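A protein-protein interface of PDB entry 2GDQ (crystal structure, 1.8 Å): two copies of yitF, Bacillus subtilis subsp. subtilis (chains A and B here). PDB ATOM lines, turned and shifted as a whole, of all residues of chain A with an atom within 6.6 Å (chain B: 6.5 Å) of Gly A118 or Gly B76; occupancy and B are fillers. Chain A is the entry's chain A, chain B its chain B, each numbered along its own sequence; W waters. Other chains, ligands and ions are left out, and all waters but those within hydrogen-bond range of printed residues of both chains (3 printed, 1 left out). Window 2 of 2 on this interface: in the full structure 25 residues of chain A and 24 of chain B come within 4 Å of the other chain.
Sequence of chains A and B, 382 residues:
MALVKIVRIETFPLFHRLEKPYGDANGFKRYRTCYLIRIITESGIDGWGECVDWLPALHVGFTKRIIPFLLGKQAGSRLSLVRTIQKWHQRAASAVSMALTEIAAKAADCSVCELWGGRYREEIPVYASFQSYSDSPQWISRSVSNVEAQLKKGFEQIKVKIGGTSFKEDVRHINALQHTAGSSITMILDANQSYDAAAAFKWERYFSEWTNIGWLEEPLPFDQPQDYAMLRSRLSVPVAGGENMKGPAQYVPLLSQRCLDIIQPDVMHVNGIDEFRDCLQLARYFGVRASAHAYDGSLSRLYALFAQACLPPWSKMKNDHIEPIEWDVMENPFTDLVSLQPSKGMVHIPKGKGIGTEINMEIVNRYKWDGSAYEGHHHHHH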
ATOM      1  N   VAL A 112     -15.240 -32.827   4.792  1.00  0.00           N
ATOM      2  CA  VAL A 112     -16.168 -32.189   5.719  1.00  0.00           C
ATOM      3  C   VAL A 112     -16.468 -30.745   5.253  1.00  0.00           C
ATOM      4  O   VAL A 112     -17.628 -30.337   5.204  1.00  0.00           O
ATOM      5  CB  VAL A 112     -15.643 -32.229   7.157  1.00  0.00           C
ATOM      6  CG1 VAL A 112     -16.557 -31.410   8.065  1.00  0.00           C
ATOM      7  CG2 VAL A 112     -15.656 -33.692   7.638  1.00  0.00           C
ATOM      8  N   CYS A 113     -15.443 -29.977   4.887  1.00  0.00           N
ATOM      9  CA  CYS A 113     -15.706 -28.582   4.454  1.00  0.00           C
ATOM     10  C   CYS A 113     -16.611 -28.511   3.218  1.00  0.00           C
ATOM     11  O   CYS A 113     -17.494 -27.642   3.144  1.00  0.00           O
ATOM     12  CB  CYS A 113     -14.415 -27.769   4.231  1.00  0.00           C
ATOM     13  SG  CYS A 113     -13.450 -27.517   5.742  1.00  0.00           S
ATOM     14  N   GLU A 114     -16.402 -29.407   2.250  1.00  0.00           N
ATOM     15  CA  GLU A 114     -17.294 -29.442   1.087  1.00  0.00           C
ATOM     16  C   GLU A 114     -18.722 -29.849   1.495  1.00  0.00           C
ATOM     17  O   GLU A 114     -19.719 -29.314   0.988  1.00  0.00           O
ATOM     18  CB  GLU A 114     -16.751 -30.380   0.009  1.00  0.00           C
ATOM     19  CG  GLU A 114     -15.441 -29.894  -0.617  1.00  0.00           C
ATOM     20  CD  GLU A 114     -14.830 -30.966  -1.536  1.00  0.00           C
ATOM     21  OE1 GLU A 114     -14.737 -32.154  -1.130  1.00  0.00           O
ATOM     22  OE2 GLU A 114     -14.460 -30.620  -2.683  1.00  0.00           O
ATOM     23  N   LEU A 115     -18.820 -30.774   2.450  1.00  0.00           N
ATOM     24  CA  LEU A 115     -20.116 -31.128   2.985  1.00  0.00           C
ATOM     25  C   LEU A 115     -20.863 -29.883   3.466  1.00  0.00           C
ATOM     26  O   LEU A 115     -22.085 -29.790   3.264  1.00  0.00           O
ATOM     27  CB  LEU A 115     -20.001 -32.158   4.107  1.00  0.00           C
ATOM     28  CG  LEU A 115     -21.326 -32.792   4.543  1.00  0.00           C
ATOM     29  CD1 LEU A 115     -21.969 -33.667   3.469  1.00  0.00           C
ATOM     30  CD2 LEU A 115     -21.082 -33.579   5.764  1.00  0.00           C
ATOM     31  N   TRP A 116     -20.127 -28.947   4.080  1.00  0.00           N
ATOM     32  CA  TRP A 116     -20.717 -27.737   4.666  1.00  0.00           C
ATOM     33  C   TRP A 116     -20.954 -26.591   3.677  1.00  0.00           C
ATOM     34  O   TRP A 116     -21.468 -25.528   4.073  1.00  0.00           O
ATOM     35  CB  TRP A 116     -19.854 -27.260   5.844  1.00  0.00           C
ATOM     36  CG  TRP A 116     -19.809 -28.198   6.998  1.00  0.00           C
ATOM     37  CD1 TRP A 116     -20.688 -29.226   7.305  1.00  0.00           C
ATOM     38  CD2 TRP A 116     -18.818 -28.200   8.025  1.00  0.00           C
ATOM     39  NE1 TRP A 116     -20.297 -29.841   8.461  1.00  0.00           N
ATOM     40  CE2 TRP A 116     -19.155 -29.231   8.929  1.00  0.00           C
ATOM     41  CE3 TRP A 116     -17.683 -27.406   8.277  1.00  0.00           C
ATOM     42  CZ2 TRP A 116     -18.391 -29.496  10.088  1.00  0.00           C
ATOM     43  CZ3 TRP A 116     -16.912 -27.687   9.409  1.00  0.00           C
ATOM     44  CH2 TRP A 116     -17.271 -28.724  10.286  1.00  0.00           C
ATOM     45  N   GLY A 117     -20.631 -26.813   2.402  1.00  0.00           N
ATOM     46  CA  GLY A 117     -20.830 -25.832   1.352  1.00  0.00           C
ATOM     47  C   GLY A 117     -19.546 -25.237   0.809  1.00  0.00           C
ATOM     48  O   GLY A 117     -19.579 -24.281   0.037  1.00  0.00           O
ATOM     49  N   GLY A 118     -18.406 -25.824   1.180  1.00  0.00           N
ATOM     50  CA  GLY A 118     -17.111 -25.389   0.669  1.00  0.00           C
ATOM     51  C   GLY A 118     -16.394 -24.375   1.555  1.00  0.00           C
ATOM     52  O   GLY A 118     -17.035 -23.575   2.233  1.00  0.00           O
ATOM     53  N   ARG A 119     -15.059 -24.410   1.570  1.00  0.00           N
ATOM     54  CA  ARG A 119     -14.348 -23.456   2.406  1.00  0.00           C
ATOM     55  C   ARG A 119     -14.221 -22.050   1.779  1.00  0.00           C
ATOM     56  O   ARG A 119     -14.360 -21.874   0.556  1.00  0.00           O
ATOM     57  CB  ARG A 119     -13.016 -24.022   2.933  1.00  0.00           C
ATOM     58  CG  ARG A 119     -11.990 -24.207   1.919  1.00  0.00           C
ATOM     59  CD  ARG A 119     -10.848 -25.148   2.354  1.00  0.00           C
ATOM     60  NE  ARG A 119     -10.335 -25.558   1.082  1.00  0.00           N
ATOM     61  CZ  ARG A 119     -10.544 -26.745   0.539  1.00  0.00           C
ATOM     62  NH1 ARG A 119     -10.099 -26.935  -0.688  1.00  0.00           N
ATOM     63  NH2 ARG A 119     -11.180 -27.727   1.219  1.00  0.00           N
ATOM     64  N   TYR A 120     -14.022 -21.045   2.626  1.00  0.00           N
ATOM     65  CA  TYR A 120     -13.654 -19.714   2.142  1.00  0.00           C
ATOM     66  C   TYR A 120     -12.137 -19.580   1.961  1.00  0.00           C
ATOM     67  O   TYR A 120     -11.689 -18.711   1.228  1.00  0.00           O
ATOM     68  CB  TYR A 120     -14.119 -18.619   3.099  1.00  0.00           C
ATOM     69  CG  TYR A 120     -15.614 -18.368   3.125  1.00  0.00           C
ATOM     70  CD1 TYR A 120     -16.242 -17.550   2.151  1.00  0.00           C
ATOM     71  CD2 TYR A 120     -16.396 -18.888   4.143  1.00  0.00           C
ATOM     72  CE1 TYR A 120     -17.629 -17.295   2.211  1.00  0.00           C
ATOM     73  CE2 TYR A 120     -17.784 -18.638   4.203  1.00  0.00           C
ATOM     74  CZ  TYR A 120     -18.395 -17.859   3.230  1.00  0.00           C
ATOM     75  OH  TYR A 120     -19.780 -17.638   3.315  1.00  0.00           O
ATOM     76  N   ARG A 121     -11.345 -20.399   2.647  1.00  0.00           N
ATOM     77  CA  ARG A 121      -9.878 -20.216   2.702  1.00  0.00           C
ATOM     78  C   ARG A 121      -9.199 -21.512   3.102  1.00  0.00           C
ATOM     79  O   ARG A 121      -9.849 -22.407   3.652  1.00  0.00           O
ATOM     80  CB  ARG A 121      -9.468 -19.088   3.678  1.00  0.00           C
ATOM     81  CG  ARG A 121      -9.693 -19.402   5.175  1.00  0.00           C
ATOM     82  CD  ARG A 121      -9.677 -18.144   6.099  1.00  0.00           C
ATOM     83  NE  ARG A 121     -10.677 -17.139   5.691  1.00  0.00           N
ATOM     84  CZ  ARG A 121     -11.971 -17.154   6.036  1.00  0.00           C
ATOM     85  NH1 ARG A 121     -12.466 -18.140   6.782  1.00  0.00           N
ATOM     86  NH2 ARG A 121     -12.789 -16.199   5.588  1.00  0.00           N
ATOM     87  N   ALA A 309     -12.459 -22.369   8.544  1.00  0.00           N
ATOM     88  CA  ALA A 309     -12.210 -22.273   7.089  1.00  0.00           C
ATOM     89  C   ALA A 309     -13.484 -22.000   6.313  1.00  0.00           C
ATOM     90  O   ALA A 309     -13.425 -21.428   5.211  1.00  0.00           O
ATOM     91  CB  ALA A 309     -11.532 -23.525   6.554  1.00  0.00           C
ATOM     92  N   CYS A 310     -14.618 -22.415   6.881  1.00  0.00           N
ATOM     93  CA  CYS A 310     -15.922 -22.192   6.262  1.00  0.00           C
ATOM     94  C   CYS A 310     -16.657 -20.937   6.794  1.00  0.00           C
ATOM     95  O   CYS A 310     -17.888 -20.789   6.587  1.00  0.00           O
ATOM     96  CB  CYS A 310     -16.787 -23.430   6.452  1.00  0.00           C
ATOM     97  SG  CYS A 310     -16.233 -24.853   5.517  1.00  0.00           S
ATOM     98  N   LEU A 311     -15.923 -20.062   7.495  1.00  0.00           N
ATOM     99  CA  LEU A 311     -16.530 -18.859   8.117  1.00  0.00           C
ATOM    100  C   LEU A 311     -16.182 -17.614   7.285  1.00  0.00           C
ATOM    101  O   LEU A 311     -15.013 -17.410   6.945  1.00  0.00           O
ATOM    102  CB  LEU A 311     -16.002 -18.669   9.535  1.00  0.00           C
ATOM    103  CG  LEU A 311     -16.730 -17.743  10.540  1.00  0.00           C
ATOM    104  CD1 LEU A 311     -18.212 -18.108  10.694  1.00  0.00           C
ATOM    105  CD2 LEU A 311     -15.982 -17.830  11.868  1.00  0.00           C
ATOM    106  N   VAL B   4     -16.115 -30.692  -9.797  1.00  0.00           N
ATOM    107  CA  VAL B   4     -16.817 -30.597 -11.099  1.00  0.00           C
ATOM    108  C   VAL B   4     -17.384 -29.172 -11.419  1.00  0.00           C
ATOM    109  O   VAL B   4     -18.330 -28.648 -10.757  1.00  0.00           O
ATOM    110  CB  VAL B   4     -17.884 -31.759 -11.253  1.00  0.00           C
ATOM    111  CG1 VAL B   4     -18.671 -31.634 -12.516  1.00  0.00           C
ATOM    112  CG2 VAL B   4     -17.203 -33.176 -11.217  1.00  0.00           C
ATOM    113  N   LYS B  73     -16.687 -22.053 -12.790  1.00  0.00           N
ATOM    114  CA  LYS B  73     -16.492 -22.085 -11.340  1.00  0.00           C
ATOM    115  C   LYS B  73     -16.773 -23.481 -10.768  1.00  0.00           C
ATOM    116  O   LYS B  73     -17.442 -24.290 -11.391  1.00  0.00           O
ATOM    117  CB  LYS B  73     -17.321 -21.020 -10.604  1.00  0.00           C
ATOM    118  CG  LYS B  73     -16.992 -19.518 -10.923  1.00  0.00           C
ATOM    119  CD  LYS B  73     -15.543 -19.150 -10.560  1.00  0.00           C
ATOM    120  CE  LYS B  73     -15.202 -17.684 -10.806  1.00  0.00           C
ATOM    121  NZ  LYS B  73     -15.419 -17.234 -12.196  1.00  0.00           N
ATOM    122  N   GLN B  74     -16.250 -23.734  -9.576  1.00  0.00           N
ATOM    123  CA  GLN B  74     -16.474 -24.993  -8.881  1.00  0.00           C
ATOM    124  C   GLN B  74     -17.854 -24.975  -8.221  1.00  0.00           C
ATOM    125  O   GLN B  74     -18.092 -24.186  -7.308  1.00  0.00           O
ATOM    126  CB  GLN B  74     -15.370 -25.227  -7.833  1.00  0.00           C
ATOM    127  CG  GLN B  74     -14.087 -25.772  -8.413  1.00  0.00           C
ATOM    128  CD  GLN B  74     -14.319 -27.117  -9.064  1.00  0.00           C
ATOM    129  OE1 GLN B  74     -14.230 -27.261 -10.290  1.00  0.00           O
ATOM    130  NE2 GLN B  74     -14.662 -28.105  -8.248  1.00  0.00           N
ATOM    131  N   ALA B  75     -18.754 -25.850  -8.678  1.00  0.00           N
ATOM    132  CA  ALA B  75     -20.115 -25.873  -8.136  1.00  0.00           C
ATOM    133  C   ALA B  75     -20.105 -26.066  -6.623  1.00  0.00           C
ATOM    134  O   ALA B  75     -21.025 -25.625  -5.947  1.00  0.00           O
ATOM    135  CB  ALA B  75     -20.958 -26.959  -8.802  1.00  0.00           C
ATOM    136  N   GLY B  76     -19.066 -26.740  -6.110  1.00  0.00           N
ATOM    137  CA  GLY B  76     -18.979 -27.095  -4.685  1.00  0.00           C
ATOM    138  C   GLY B  76     -18.639 -25.973  -3.723  1.00  0.00           C
ATOM    139  O   GLY B  76     -18.851 -26.110  -2.500  1.00  0.00           O
ATOM    140  N   SER B  77     -18.097 -24.882  -4.262  1.00  0.00           N
ATOM    141  CA  SER B  77     -17.760 -23.702  -3.468  1.00  0.00           C
ATOM    142  C   SER B  77     -19.026 -22.853  -3.299  1.00  0.00           C
ATOM    143  O   SER B  77     -19.084 -21.705  -3.734  1.00  0.00           O
ATOM    144  CB  SER B  77     -16.634 -22.873  -4.138  1.00  0.00           C
ATOM    145  OG  SER B  77     -15.431 -23.637  -4.294  1.00  0.00           O
ATOM    146  N   ARG B  78     -20.049 -23.458  -2.695  1.00  0.00           N
ATOM    147  CA  ARG B  78     -21.359 -22.825  -2.593  1.00  0.00           C
ATOM    148  C   ARG B  78     -21.345 -21.560  -1.721  1.00  0.00           C
ATOM    149  O   ARG B  78     -21.865 -20.530  -2.134  1.00  0.00           O
ATOM    150  CB  ARG B  78     -22.448 -23.822  -2.156  1.00  0.00           C
ATOM    151  CG  ARG B  78     -23.875 -23.204  -2.038  1.00  0.00           C
ATOM    152  CD  ARG B  78     -24.939 -24.219  -1.656  1.00  0.00           C
ATOM    153  NE  ARG B  78     -24.909 -24.519  -0.217  1.00  0.00           N
ATOM    154  CZ  ARG B  78     -24.459 -25.649   0.333  1.00  0.00           C
ATOM    155  NH1 ARG B  78     -23.990 -26.641  -0.425  1.00  0.00           N
ATOM    156  NH2 ARG B  78     -24.509 -25.788   1.678  1.00  0.00           N
ATOM    157  N   LEU B  79     -20.716 -21.621  -0.555  1.00  0.00           N
ATOM    158  CA  LEU B  79     -20.787 -20.485   0.385  1.00  0.00           C
ATOM    159  C   LEU B  79     -20.164 -19.256  -0.273  1.00  0.00           C
ATOM    160  O   LEU B  79     -20.790 -18.175  -0.327  1.00  0.00           O
ATOM    161  CB  LEU B  79     -20.126 -20.816   1.739  1.00  0.00           C
ATOM    162  CG  LEU B  79     -20.825 -21.922   2.562  1.00  0.00           C
ATOM    163  CD1 LEU B  79     -20.173 -22.168   3.932  1.00  0.00           C
ATOM    164  CD2 LEU B  79     -22.298 -21.625   2.737  1.00  0.00           C
ATOM    165  N   SER B  80     -18.975 -19.463  -0.843  1.00  0.00           N
ATOM    166  CA  SER B  80     -18.166 -18.419  -1.501  1.00  0.00           C
ATOM    167  C   SER B  80     -18.867 -17.777  -2.695  1.00  0.00           C
ATOM    168  O   SER B  80     -18.978 -16.555  -2.760  1.00  0.00           O
ATOM    169  CB  SER B  80     -16.800 -18.988  -1.956  1.00  0.00           C
ATOM    170  OG  SER B  80     -16.047 -17.952  -2.590  1.00  0.00           O
ATOM    171  N   LEU B  81     -19.313 -18.605  -3.641  1.00  0.00           N
ATOM    172  CA  LEU B  81     -20.042 -18.148  -4.839  1.00  0.00           C
ATOM    173  C   LEU B  81     -21.326 -17.388  -4.513  1.00  0.00           C
ATOM    174  O   LEU B  81     -21.622 -16.360  -5.145  1.00  0.00           O
ATOM    175  CB  LEU B  81     -20.361 -19.319  -5.784  1.00  0.00           C
ATOM    176  CG  LEU B  81     -19.162 -20.028  -6.448  1.00  0.00           C
ATOM    177  CD1 LEU B  81     -19.708 -21.210  -7.249  1.00  0.00           C
ATOM    178  CD2 LEU B  81     -18.335 -19.072  -7.325  1.00  0.00           C
ATOM    179  N   LEU B 100     -27.158 -24.843  -6.645  1.00  0.00           N
ATOM    180  CA  LEU B 100     -25.922 -25.442  -6.134  1.00  0.00           C
ATOM    181  C   LEU B 100     -26.193 -26.500  -5.049  1.00  0.00           C
ATOM    182  O   LEU B 100     -25.470 -27.521  -4.972  1.00  0.00           O
ATOM    183  CB  LEU B 100     -24.911 -24.388  -5.646  1.00  0.00           C
ATOM    184  CG  LEU B 100     -24.454 -23.364  -6.709  1.00  0.00           C
ATOM    185  CD1 LEU B 100     -23.440 -22.339  -6.146  1.00  0.00           C
ATOM    186  CD2 LEU B 100     -23.935 -24.061  -7.974  1.00  0.00           C
ATOM    187  N   ILE B 103     -27.238 -29.685  -6.798  1.00  0.00           N
ATOM    188  CA  ILE B 103     -26.016 -30.290  -7.372  1.00  0.00           C
ATOM    189  C   ILE B 103     -25.235 -31.075  -6.302  1.00  0.00           C
ATOM    190  O   ILE B 103     -24.930 -32.280  -6.484  1.00  0.00           O
ATOM    191  CB  ILE B 103     -25.161 -29.223  -8.072  1.00  0.00           C
ATOM    192  CG1 ILE B 103     -25.845 -28.852  -9.406  1.00  0.00           C
ATOM    193  CG2 ILE B 103     -23.718 -29.702  -8.262  1.00  0.00           C
ATOM    194  CD1 ILE B 103     -25.421 -27.509 -10.021  1.00  0.00           C
ATOM    195  N   ALA B 104     -24.967 -30.396  -5.183  1.00  0.00           N
ATOM    196  CA  ALA B 104     -24.307 -31.005  -4.032  1.00  0.00           C
ATOM    197  C   ALA B 104     -24.973 -32.308  -3.576  1.00  0.00           C
ATOM    198  O   ALA B 104     -24.277 -33.303  -3.379  1.00  0.00           O
ATOM    199  CB  ALA B 104     -24.220 -29.988  -2.863  1.00  0.00           C
HETATM  200  O   HOH W   1     -24.692 -28.143   3.475  1.00  0.00           O
HETATM  201  O   HOH W   2     -22.877 -29.088   0.528  1.00  0.00           O
HETATM  202  O   HOH W   3     -20.019 -28.315  -1.659  1.00  0.00           O
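Trp A116 touches Arg B78 (O to NH2, 3.9 Å).
Trp A116 touches Leu B79 (O to CD1, 3.6 Å).
Ser B77 touches Gly A117 (C to O, 3.7 Å).
Gly A118 touches Gly B76.
CD1 of Leu B79 touches O of Gly A118, 3.8 Å away.
OH of Tyr A120 touches CB of Leu B79, at 3.6 Å.
CA of Ser B80 touches CE1 of Tyr A120, 3.9 Å away.
Cys A310 touches Leu B79 (O to CD1, 3.8 Å).
The backbone NH (N) of Gly A118 lies within hydrogen-bond range of the backbone carbonyl oxygen (O) of Cys A113 (2.8 Å).
The backbone carbonyl oxygen (O) of Gly A118 lies within hydrogen-bond range of the side-chain sulfur (SG) of Cys A310, at 3.6 Å.
The backbone carbonyl oxygen of Ala A309 sits at hydrogen-bond distance from the backbone NH of Tyr A120 (2.7 Å).
Water W3 bridges O of Gly B76 and O of Glu A114.
Water W2 lies within hydrogen-bond range of the guanidinium group of Arg B78 (2.9 Å), the backbone carbonyl oxygen of Leu A115 (2.9 Å) and the backbone carbonyl oxygen of Glu A114 (3.2 Å).
Water W1 bridges NH2 of Arg B78 (3.0 Å) and O of Leu A115 (3.1 Å).
Of the 13 printed residues of chain B, 5 touch a printed residue of chain A.
Hydrophobic or aromatic side chains of chain B within 4 Å of the printed part of chain A: Leu B79.
Hydrophobic or aromatic side chains of chain A within 4 Å of the printed part of chain B: Tyr A120.
Among the printed residues, no Asp or Glu carboxylate lies within 4 Å of a Lys or Arg side-chain nitrogen of the other chain.
The backbone carbonyl oxygen (O) of Gly A117 lies within hydrogen-bond range of the backbone NH (N) of Arg B78, at 2.9 Å.
The backbone NH of Leu B79 is in hydrogen-bond range of the backbone carbonyl oxygen of Gly A117, 3.0 Å away.
O of Gly B76 lies close to O of Gly A117, 3.2 Å away.
Gly A118 touches just these residues of chain B: Gly B76 and Leu B79.
Of the printed residues of chain A, Gly B76 touches Gly A117 (3.2 Å) and Gly A118 (3.7 Å).
Printed residues of chain B within 4 Å of Cys A310: Leu B79 (3.8 Å).
Of the printed residues of chain A, Ser B80 touches Tyr A120.
Val B4 touches none of the printed residues of chain A.
The nearest residue of chain B that does not touch Gly A118 is Ser B77 (4.5 Å).
No position is printed for both chains.
Of the 11 pairs that touch across the chains among the printed residues, none has its exchanged pair printed and touching as well.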
